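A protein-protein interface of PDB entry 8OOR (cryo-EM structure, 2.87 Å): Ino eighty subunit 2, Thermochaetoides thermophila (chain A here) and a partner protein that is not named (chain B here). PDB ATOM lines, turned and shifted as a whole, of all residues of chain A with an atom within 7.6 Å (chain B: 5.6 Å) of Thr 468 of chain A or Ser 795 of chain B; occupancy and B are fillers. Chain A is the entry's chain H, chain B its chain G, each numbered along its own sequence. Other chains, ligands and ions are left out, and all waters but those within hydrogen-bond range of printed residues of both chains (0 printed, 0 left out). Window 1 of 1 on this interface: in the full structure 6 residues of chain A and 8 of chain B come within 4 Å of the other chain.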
ATOM      1  N   PRO A 445      20.165  26.005  28.529  1.00  0.00           N
ATOM      2  CA  PRO A 445      19.871  24.615  28.904  1.00  0.00           C
ATOM      3  C   PRO A 445      20.785  23.563  28.304  1.00  0.00           C
ATOM      4  O   PRO A 445      20.935  22.493  28.900  1.00  0.00           O
ATOM      5  CB  PRO A 445      18.441  24.435  28.388  1.00  0.00           C
ATOM      6  CG  PRO A 445      17.858  25.769  28.504  1.00  0.00           C
ATOM      7  CD  PRO A 445      18.952  26.716  28.103  1.00  0.00           C
ATOM      8  N   MET A 446      21.389  23.816  27.146  1.00  0.00           N
ATOM      9  CA  MET A 446      22.184  22.803  26.467  1.00  0.00           C
ATOM     10  C   MET A 446      23.689  22.917  26.650  1.00  0.00           C
ATOM     11  O   MET A 446      24.404  22.023  26.196  1.00  0.00           O
ATOM     12  CB  MET A 446      21.865  22.792  24.972  1.00  0.00           C
ATOM     13  CG  MET A 446      20.515  22.180  24.656  1.00  0.00           C
ATOM     14  SD  MET A 446      20.346  21.697  22.930  1.00  0.00           S
ATOM     15  CE  MET A 446      20.335  23.292  22.132  1.00  0.00           C
ATOM     16  N   VAL A 461      27.006  22.498  35.306  1.00  0.00           N
ATOM     17  CA  VAL A 461      26.080  21.764  34.456  1.00  0.00           C
ATOM     18  C   VAL A 461      24.685  22.332  34.680  1.00  0.00           C
ATOM     19  O   VAL A 461      24.273  22.491  35.828  1.00  0.00           O
ATOM     20  CB  VAL A 461      26.086  20.255  34.750  1.00  0.00           C
ATOM     21  CG1 VAL A 461      25.255  19.513  33.733  1.00  0.00           C
ATOM     22  CG2 VAL A 461      27.478  19.745  34.786  1.00  0.00           C
ATOM     23  N   PRO A 462      23.949  22.677  33.628  1.00  0.00           N
ATOM     24  CA  PRO A 462      22.559  23.106  33.798  1.00  0.00           C
ATOM     25  C   PRO A 462      21.720  22.034  34.465  1.00  0.00           C
ATOM     26  O   PRO A 462      21.846  20.847  34.165  1.00  0.00           O
ATOM     27  CB  PRO A 462      22.090  23.350  32.365  1.00  0.00           C
ATOM     28  CG  PRO A 462      23.293  23.605  31.615  1.00  0.00           C
ATOM     29  CD  PRO A 462      24.371  22.771  32.227  1.00  0.00           C
ATOM     30  N   GLU A 463      20.828  22.468  35.354  1.00  0.00           N
ATOM     31  CA  GLU A 463      19.887  21.540  35.963  1.00  0.00           C
ATOM     32  C   GLU A 463      18.944  20.925  34.941  1.00  0.00           C
ATOM     33  O   GLU A 463      18.364  19.868  35.201  1.00  0.00           O
ATOM     34  CB  GLU A 463      19.091  22.256  37.045  1.00  0.00           C
ATOM     35  CG  GLU A 463      18.181  23.330  36.504  1.00  0.00           C
ATOM     36  CD  GLU A 463      17.669  24.252  37.589  1.00  0.00           C
ATOM     37  OE1 GLU A 463      17.841  23.916  38.777  1.00  0.00           O
ATOM     38  OE2 GLU A 463      17.099  25.315  37.256  1.00  0.00           O
ATOM     39  N   GLU A 464      18.791  21.551  33.779  1.00  0.00           N
ATOM     40  CA  GLU A 464      18.089  20.922  32.672  1.00  0.00           C
ATOM     41  C   GLU A 464      18.837  19.725  32.105  1.00  0.00           C
ATOM     42  O   GLU A 464      18.223  18.905  31.417  1.00  0.00           O
ATOM     43  CB  GLU A 464      17.833  21.938  31.563  1.00  0.00           C
ATOM     44  CG  GLU A 464      16.933  23.081  31.977  1.00  0.00           C
ATOM     45  CD  GLU A 464      17.682  24.181  32.699  1.00  0.00           C
ATOM     46  OE1 GLU A 464      18.898  24.024  32.929  1.00  0.00           O
ATOM     47  OE2 GLU A 464      17.051  25.198  33.048  1.00  0.00           O
ATOM     48  N   LEU A 465      20.144  19.617  32.348  1.00  0.00           N
ATOM     49  CA  LEU A 465      20.910  18.477  31.863  1.00  0.00           C
ATOM     50  C   LEU A 465      21.116  17.379  32.890  1.00  0.00           C
ATOM     51  O   LEU A 465      21.323  16.228  32.497  1.00  0.00           O
ATOM     52  CB  LEU A 465      22.291  18.928  31.387  1.00  0.00           C
ATOM     53  CG  LEU A 465      22.378  19.695  30.080  1.00  0.00           C
ATOM     54  CD1 LEU A 465      23.807  20.129  29.863  1.00  0.00           C
ATOM     55  CD2 LEU A 465      21.883  18.830  28.944  1.00  0.00           C
ATOM     56  N   LEU A 466      21.051  17.689  34.176  1.00  0.00           N
ATOM     57  CA  LEU A 466      20.949  16.642  35.177  1.00  0.00           C
ATOM     58  C   LEU A 466      19.672  15.847  34.966  1.00  0.00           C
ATOM     59  O   LEU A 466      18.621  16.402  34.645  1.00  0.00           O
ATOM     60  CB  LEU A 466      20.992  17.239  36.576  1.00  0.00           C
ATOM     61  CG  LEU A 466      22.173  18.175  36.808  1.00  0.00           C
ATOM     62  CD1 LEU A 466      22.272  18.569  38.265  1.00  0.00           C
ATOM     63  CD2 LEU A 466      23.447  17.509  36.369  1.00  0.00           C
ATOM     64  N   GLY A 467      19.764  14.537  35.134  1.00  0.00           N
ATOM     65  CA  GLY A 467      18.673  13.669  34.767  1.00  0.00           C
ATOM     66  C   GLY A 467      18.624  13.302  33.306  1.00  0.00           C
ATOM     67  O   GLY A 467      17.680  12.626  32.886  1.00  0.00           O
ATOM     68  N   THR A 468      19.580  13.761  32.513  1.00  0.00           N
ATOM     69  CA  THR A 468      19.804  13.266  31.169  1.00  0.00           C
ATOM     70  C   THR A 468      21.038  12.372  31.160  1.00  0.00           C
ATOM     71  O   THR A 468      21.735  12.227  32.162  1.00  0.00           O
ATOM     72  CB  THR A 468      19.953  14.426  30.191  1.00  0.00           C
ATOM     73  OG1 THR A 468      21.252  14.996  30.351  1.00  0.00           O
ATOM     74  CG2 THR A 468      18.907  15.482  30.458  1.00  0.00           C
ATOM     75  N   HIS A 469      21.315  11.767  30.006  1.00  0.00           N
ATOM     76  CA  HIS A 469      22.546  10.999  29.852  1.00  0.00           C
ATOM     77  C   HIS A 469      23.788  11.845  30.079  1.00  0.00           C
ATOM     78  O   HIS A 469      24.822  11.324  30.503  1.00  0.00           O
ATOM     79  CB  HIS A 469      22.580  10.354  28.471  1.00  0.00           C
ATOM     80  CG  HIS A 469      22.889  11.312  27.365  1.00  0.00           C
ATOM     81  ND1 HIS A 469      24.163  11.759  27.096  1.00  0.00           N
ATOM     82  CD2 HIS A 469      22.084  11.899  26.450  1.00  0.00           C
ATOM     83  CE1 HIS A 469      24.128  12.590  26.073  1.00  0.00           C
ATOM     84  NE2 HIS A 469      22.878  12.692  25.662  1.00  0.00           N
ATOM     85  N   ALA A 470      23.715  13.141  29.787  1.00  0.00           N
ATOM     86  CA  ALA A 470      24.850  14.027  30.015  1.00  0.00           C
ATOM     87  C   ALA A 470      25.164  14.211  31.491  1.00  0.00           C
ATOM     88  O   ALA A 470      26.299  14.544  31.840  1.00  0.00           O
ATOM     89  CB  ALA A 470      24.586  15.381  29.370  1.00  0.00           C
ATOM     90  N   GLY A 471      24.177  14.049  32.366  1.00  0.00           N
ATOM     91  CA  GLY A 471      24.415  14.156  33.794  1.00  0.00           C
ATOM     92  C   GLY A 471      25.189  13.013  34.409  1.00  0.00           C
ATOM     93  O   GLY A 471      25.788  13.194  35.471  1.00  0.00           O
ATOM     94  N   VAL A 472      25.207  11.851  33.756  1.00  0.00           N
ATOM     95  CA  VAL A 472      25.765  10.638  34.349  1.00  0.00           C
ATOM     96  C   VAL A 472      27.211  10.834  34.775  1.00  0.00           C
ATOM     97  O   VAL A 472      27.605  10.428  35.873  1.00  0.00           O
ATOM     98  CB  VAL A 472      25.633   9.465  33.364  1.00  0.00           C
ATOM     99  CG1 VAL A 472      26.311   8.238  33.911  1.00  0.00           C
ATOM    100  CG2 VAL A 472      24.187   9.185  33.068  1.00  0.00           C
ATOM    101  N   VAL A 473      28.022  11.463  33.926  1.00  0.00           N
ATOM    102  CA  VAL A 473      29.431  11.665  34.245  1.00  0.00           C
ATOM    103  C   VAL A 473      29.596  12.531  35.480  1.00  0.00           C
ATOM    104  O   VAL A 473      30.562  12.379  36.232  1.00  0.00           O
ATOM    105  CB  VAL A 473      30.156  12.266  33.027  1.00  0.00           C
ATOM    106  CG1 VAL A 473      31.624  12.462  33.313  1.00  0.00           C
ATOM    107  CG2 VAL A 473      29.977  11.372  31.830  1.00  0.00           C
ATOM    108  N   PHE A 474      28.664  13.433  35.721  1.00  0.00           N
ATOM    109  CA  PHE A 474      28.671  14.262  36.912  1.00  0.00           C
ATOM    110  C   PHE A 474      27.982  13.592  38.093  1.00  0.00           C
ATOM    111  O   PHE A 474      27.832  14.216  39.145  1.00  0.00           O
ATOM    112  CB  PHE A 474      28.022  15.601  36.590  1.00  0.00           C
ATOM    113  CG  PHE A 474      28.568  16.239  35.354  1.00  0.00           C
ATOM    114  CD1 PHE A 474      29.788  16.878  35.375  1.00  0.00           C
ATOM    115  CD2 PHE A 474      27.899  16.129  34.155  1.00  0.00           C
ATOM    116  CE1 PHE A 474      30.297  17.443  34.240  1.00  0.00           C
ATOM    117  CE2 PHE A 474      28.409  16.687  33.020  1.00  0.00           C
ATOM    118  CZ  PHE A 474      29.605  17.350  33.065  1.00  0.00           C
ATOM    119  N   ALA A 476      24.780  12.306  38.092  1.00  0.00           N
ATOM    120  CA  ALA A 476      23.428  12.834  38.182  1.00  0.00           C
ATOM    121  C   ALA A 476      22.623  12.423  36.953  1.00  0.00           C
ATOM    122  O   ALA A 476      21.917  13.229  36.346  1.00  0.00           O
ATOM    123  CB  ALA A 476      23.456  14.352  38.352  1.00  0.00           C
ATOM    124  N   GLY A 477      22.694  11.154  36.580  1.00  0.00           N
ATOM    125  CA  GLY A 477      21.936  10.660  35.456  1.00  0.00           C
ATOM    126  C   GLY A 477      20.450  10.547  35.708  1.00  0.00           C
ATOM    127  O   GLY A 477      19.918  11.077  36.686  1.00  0.00           O
ATOM    128  N   PRO A 478      19.736   9.874  34.796  1.00  0.00           N
ATOM    129  CA  PRO A 478      18.300   9.607  34.912  1.00  0.00           C
ATOM    130  C   PRO A 478      17.918   8.937  36.230  1.00  0.00           C
ATOM    131  O   PRO A 478      18.716   8.167  36.761  1.00  0.00           O
ATOM    132  CB  PRO A 478      18.023   8.667  33.736  1.00  0.00           C
ATOM    133  CG  PRO A 478      19.099   8.948  32.770  1.00  0.00           C
ATOM    134  CD  PRO A 478      20.306   9.266  33.587  1.00  0.00           C
ATOM    135  N   GLU B 790      17.251  17.429  16.297  1.00  0.00           N
ATOM    136  CA  GLU B 790      18.062  16.246  16.551  1.00  0.00           C
ATOM    137  C   GLU B 790      19.130  16.500  17.595  1.00  0.00           C
ATOM    138  O   GLU B 790      19.421  15.626  18.415  1.00  0.00           O
ATOM    139  CB  GLU B 790      18.700  15.786  15.254  1.00  0.00           C
ATOM    140  CG  GLU B 790      17.713  15.215  14.299  1.00  0.00           C
ATOM    141  CD  GLU B 790      18.320  14.931  12.955  1.00  0.00           C
ATOM    142  OE1 GLU B 790      19.322  15.585  12.605  1.00  0.00           O
ATOM    143  OE2 GLU B 790      17.781  14.074  12.231  1.00  0.00           O
ATOM    144  N   ILE B 791      19.727  17.683  17.589  1.00  0.00           N
ATOM    145  CA  ILE B 791      20.697  18.000  18.625  1.00  0.00           C
ATOM    146  C   ILE B 791      20.036  18.055  19.996  1.00  0.00           C
ATOM    147  O   ILE B 791      20.628  17.636  20.996  1.00  0.00           O
ATOM    148  CB  ILE B 791      21.418  19.310  18.278  1.00  0.00           C
ATOM    149  CG1 ILE B 791      22.260  19.115  17.021  1.00  0.00           C
ATOM    150  CG2 ILE B 791      22.335  19.714  19.403  1.00  0.00           C
ATOM    151  CD1 ILE B 791      22.620  20.406  16.338  1.00  0.00           C
ATOM    152  N   LYS B 792      18.812  18.581  20.076  1.00  0.00           N
ATOM    153  CA  LYS B 792      18.067  18.538  21.333  1.00  0.00           C
ATOM    154  C   LYS B 792      17.732  17.113  21.758  1.00  0.00           C
ATOM    155  O   LYS B 792      17.997  16.719  22.897  1.00  0.00           O
ATOM    156  CB  LYS B 792      16.797  19.374  21.230  1.00  0.00           C
ATOM    157  CG  LYS B 792      17.055  20.858  21.280  1.00  0.00           C
ATOM    158  CD  LYS B 792      15.763  21.636  21.182  1.00  0.00           C
ATOM    159  CE  LYS B 792      16.021  23.126  21.249  1.00  0.00           C
ATOM    160  NZ  LYS B 792      14.753  23.907  21.189  1.00  0.00           N
ATOM    161  N   GLU B 793      17.154  16.319  20.856  1.00  0.00           N
ATOM    162  CA  GLU B 793      16.812  14.943  21.203  1.00  0.00           C
ATOM    163  C   GLU B 793      18.045  14.140  21.588  1.00  0.00           C
ATOM    164  O   GLU B 793      17.997  13.312  22.502  1.00  0.00           O
ATOM    165  CB  GLU B 793      16.090  14.265  20.043  1.00  0.00           C
ATOM    166  CG  GLU B 793      14.673  14.746  19.822  1.00  0.00           C
ATOM    167  CD  GLU B 793      14.047  14.165  18.564  1.00  0.00           C
ATOM    168  OE1 GLU B 793      14.681  13.296  17.926  1.00  0.00           O
ATOM    169  OE2 GLU B 793      12.924  14.582  18.208  1.00  0.00           O
ATOM    170  N   ALA B 794      19.155  14.362  20.898  1.00  0.00           N
ATOM    171  CA  ALA B 794      20.395  13.705  21.276  1.00  0.00           C
ATOM    172  C   ALA B 794      20.918  14.186  22.621  1.00  0.00           C
ATOM    173  O   ALA B 794      21.630  13.443  23.302  1.00  0.00           O
ATOM    174  CB  ALA B 794      21.454  13.916  20.200  1.00  0.00           C
ATOM    175  N   SER B 795      20.610  15.416  23.013  1.00  0.00           N
ATOM    176  CA  SER B 795      21.204  15.956  24.225  1.00  0.00           C
ATOM    177  C   SER B 795      20.365  15.788  25.484  1.00  0.00           C
ATOM    178  O   SER B 795      20.936  15.670  26.571  1.00  0.00           O
ATOM    179  CB  SER B 795      21.498  17.438  24.028  1.00  0.00           C
ATOM    180  OG  SER B 795      20.317  18.113  23.653  1.00  0.00           O
ATOM    181  N   PHE B 796      19.040  15.805  25.391  1.00  0.00           N
ATOM    182  CA  PHE B 796      18.203  15.691  26.581  1.00  0.00           C
ATOM    183  C   PHE B 796      17.739  14.278  26.897  1.00  0.00           C
ATOM    184  O   PHE B 796      17.156  14.069  27.963  1.00  0.00           O
ATOM    185  CB  PHE B 796      16.986  16.602  26.465  1.00  0.00           C
ATOM    186  CG  PHE B 796      17.326  18.047  26.516  1.00  0.00           C
ATOM    187  CD1 PHE B 796      17.876  18.588  27.649  1.00  0.00           C
ATOM    188  CD2 PHE B 796      17.110  18.862  25.432  1.00  0.00           C
ATOM    189  CE1 PHE B 796      18.193  19.912  27.707  1.00  0.00           C
ATOM    190  CE2 PHE B 796      17.428  20.189  25.488  1.00  0.00           C
ATOM    191  CZ  PHE B 796      17.969  20.713  26.627  1.00  0.00           C
ATOM    192  N   GLY B 797      17.984  13.312  26.025  1.00  0.00           N
ATOM    193  CA  GLY B 797      17.540  11.957  26.249  1.00  0.00           C
ATOM    194  C   GLY B 797      18.142  11.316  27.484  1.00  0.00           C
ATOM    195  O   GLY B 797      19.150  11.774  28.028  1.00  0.00           O
ATOM    196  N   PRO B 798      17.501  10.254  27.975  1.00  0.00           N
ATOM    197  CA  PRO B 798      18.059   9.541  29.129  1.00  0.00           C
ATOM    198  C   PRO B 798      19.300   8.746  28.787  1.00  0.00           C
ATOM    199  O   PRO B 798      20.129   8.505  29.670  1.00  0.00           O
ATOM    200  CB  PRO B 798      16.907   8.626  29.555  1.00  0.00           C
ATOM    201  CG  PRO B 798      16.186   8.362  28.293  1.00  0.00           C
ATOM    202  CD  PRO B 798      16.258   9.630  27.495  1.00  0.00           C
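A ring nitrogen (NE2) of His 469 of chain A lies within hydrogen-bond range of the backbone carbonyl oxygen of Ala 794 of chain B (2.8 Å).
OG of Ser 795 of chain B sits at hydrogen-bond distance from SD of Met 446 of chain A (3.7 Å).
O of Gly 797 of chain B lies within hydrogen-bond range of N of His 469 of chain A (2.9 Å).
N of His 469 of chain A sits close to O of Pro 798 of chain B (3.5 Å).
OG of Ser 795 of chain B is in hydrogen-bond range of O of Ile 791 of chain B, 2.7 Å away.
O of Lys 792 of chain B sits at hydrogen-bond distance from OG of Ser 795 of chain B (2.8 Å).
O of Leu 465 of chain A sits at hydrogen-bond distance from OG1 of Thr 468 of chain A (2.5 Å).
The side-chain hydroxyl (OG1) of Thr 468 of chain A lies close to the backbone NH (N) of Ala 470 of chain A (3.1 Å).
Pro 445 of chain A touches Phe 796 of chain B.
CG of Lys 792 of chain B touches SD of Met 446 of chain A (3.8 Å).
Met 446 of chain A touches Phe 796 of chain B (CG to CZ, 3.5 Å).
Glu 464 of chain A touches Phe 796 of chain B (O to CD1, 3.8 Å).
Thr 468 of chain A touches Ser 795 of chain B.
CG2 of Thr 468 of chain A touches O of Phe 796 of chain B, at 3.4 Å.
Gly 797 of chain B touches Thr 468 of chain A (O to CB, 3.5 Å).
Ser 795 of chain B touches His 469 of chain A.
Pro 478 of chain A touches Pro 798 of chain B (CG to O, 3.3 Å).
Of chain B, only Ser 795 (3.9 Å), Phe 796 (3.4 Å) and Gly 797 (3.5 Å) come within 4 Å of Thr 468 of chain A.
Of chain A, only Met 446, Thr 468 and His 469 come within 4 Å of Ser 795 of chain B.
Ala 794 of chain B touches just one residue of chain A: His 469 (2.8 Å).
Printed residues of chain B within 4 Å of His 469 of chain A: Ala 794, Ser 795, Gly 797 and Pro 798.
Printed residues of chain B within 4 Å of Met 446 of chain A: Lys 792 (3.8 Å), Ser 795 (3.7 Å) and Phe 796 (3.5 Å).
Of the printed residues of chain A, Pro 798 of chain B touches His 469 (3.3 Å) and Pro 478 (3.3 Å).
The nearest residue of chain A that does not touch Ser 795 of chain B is Leu 465 of chain A (4.1 Å).
Hydrophobic or aromatic side chains of chain B within 4 Å of the printed part of chain A: Phe 796 and Pro 798.
Hydrophobic or aromatic side chains of chain A that line the printed part of chain B: Met 446, His 469 and Pro 478.
Among the printed residues, 13 pairs touch across the chains.
Among the printed residues, no Asp or Glu carboxylate lies within 4 Å of a Lys or Arg side-chain nitrogen of the other chain.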
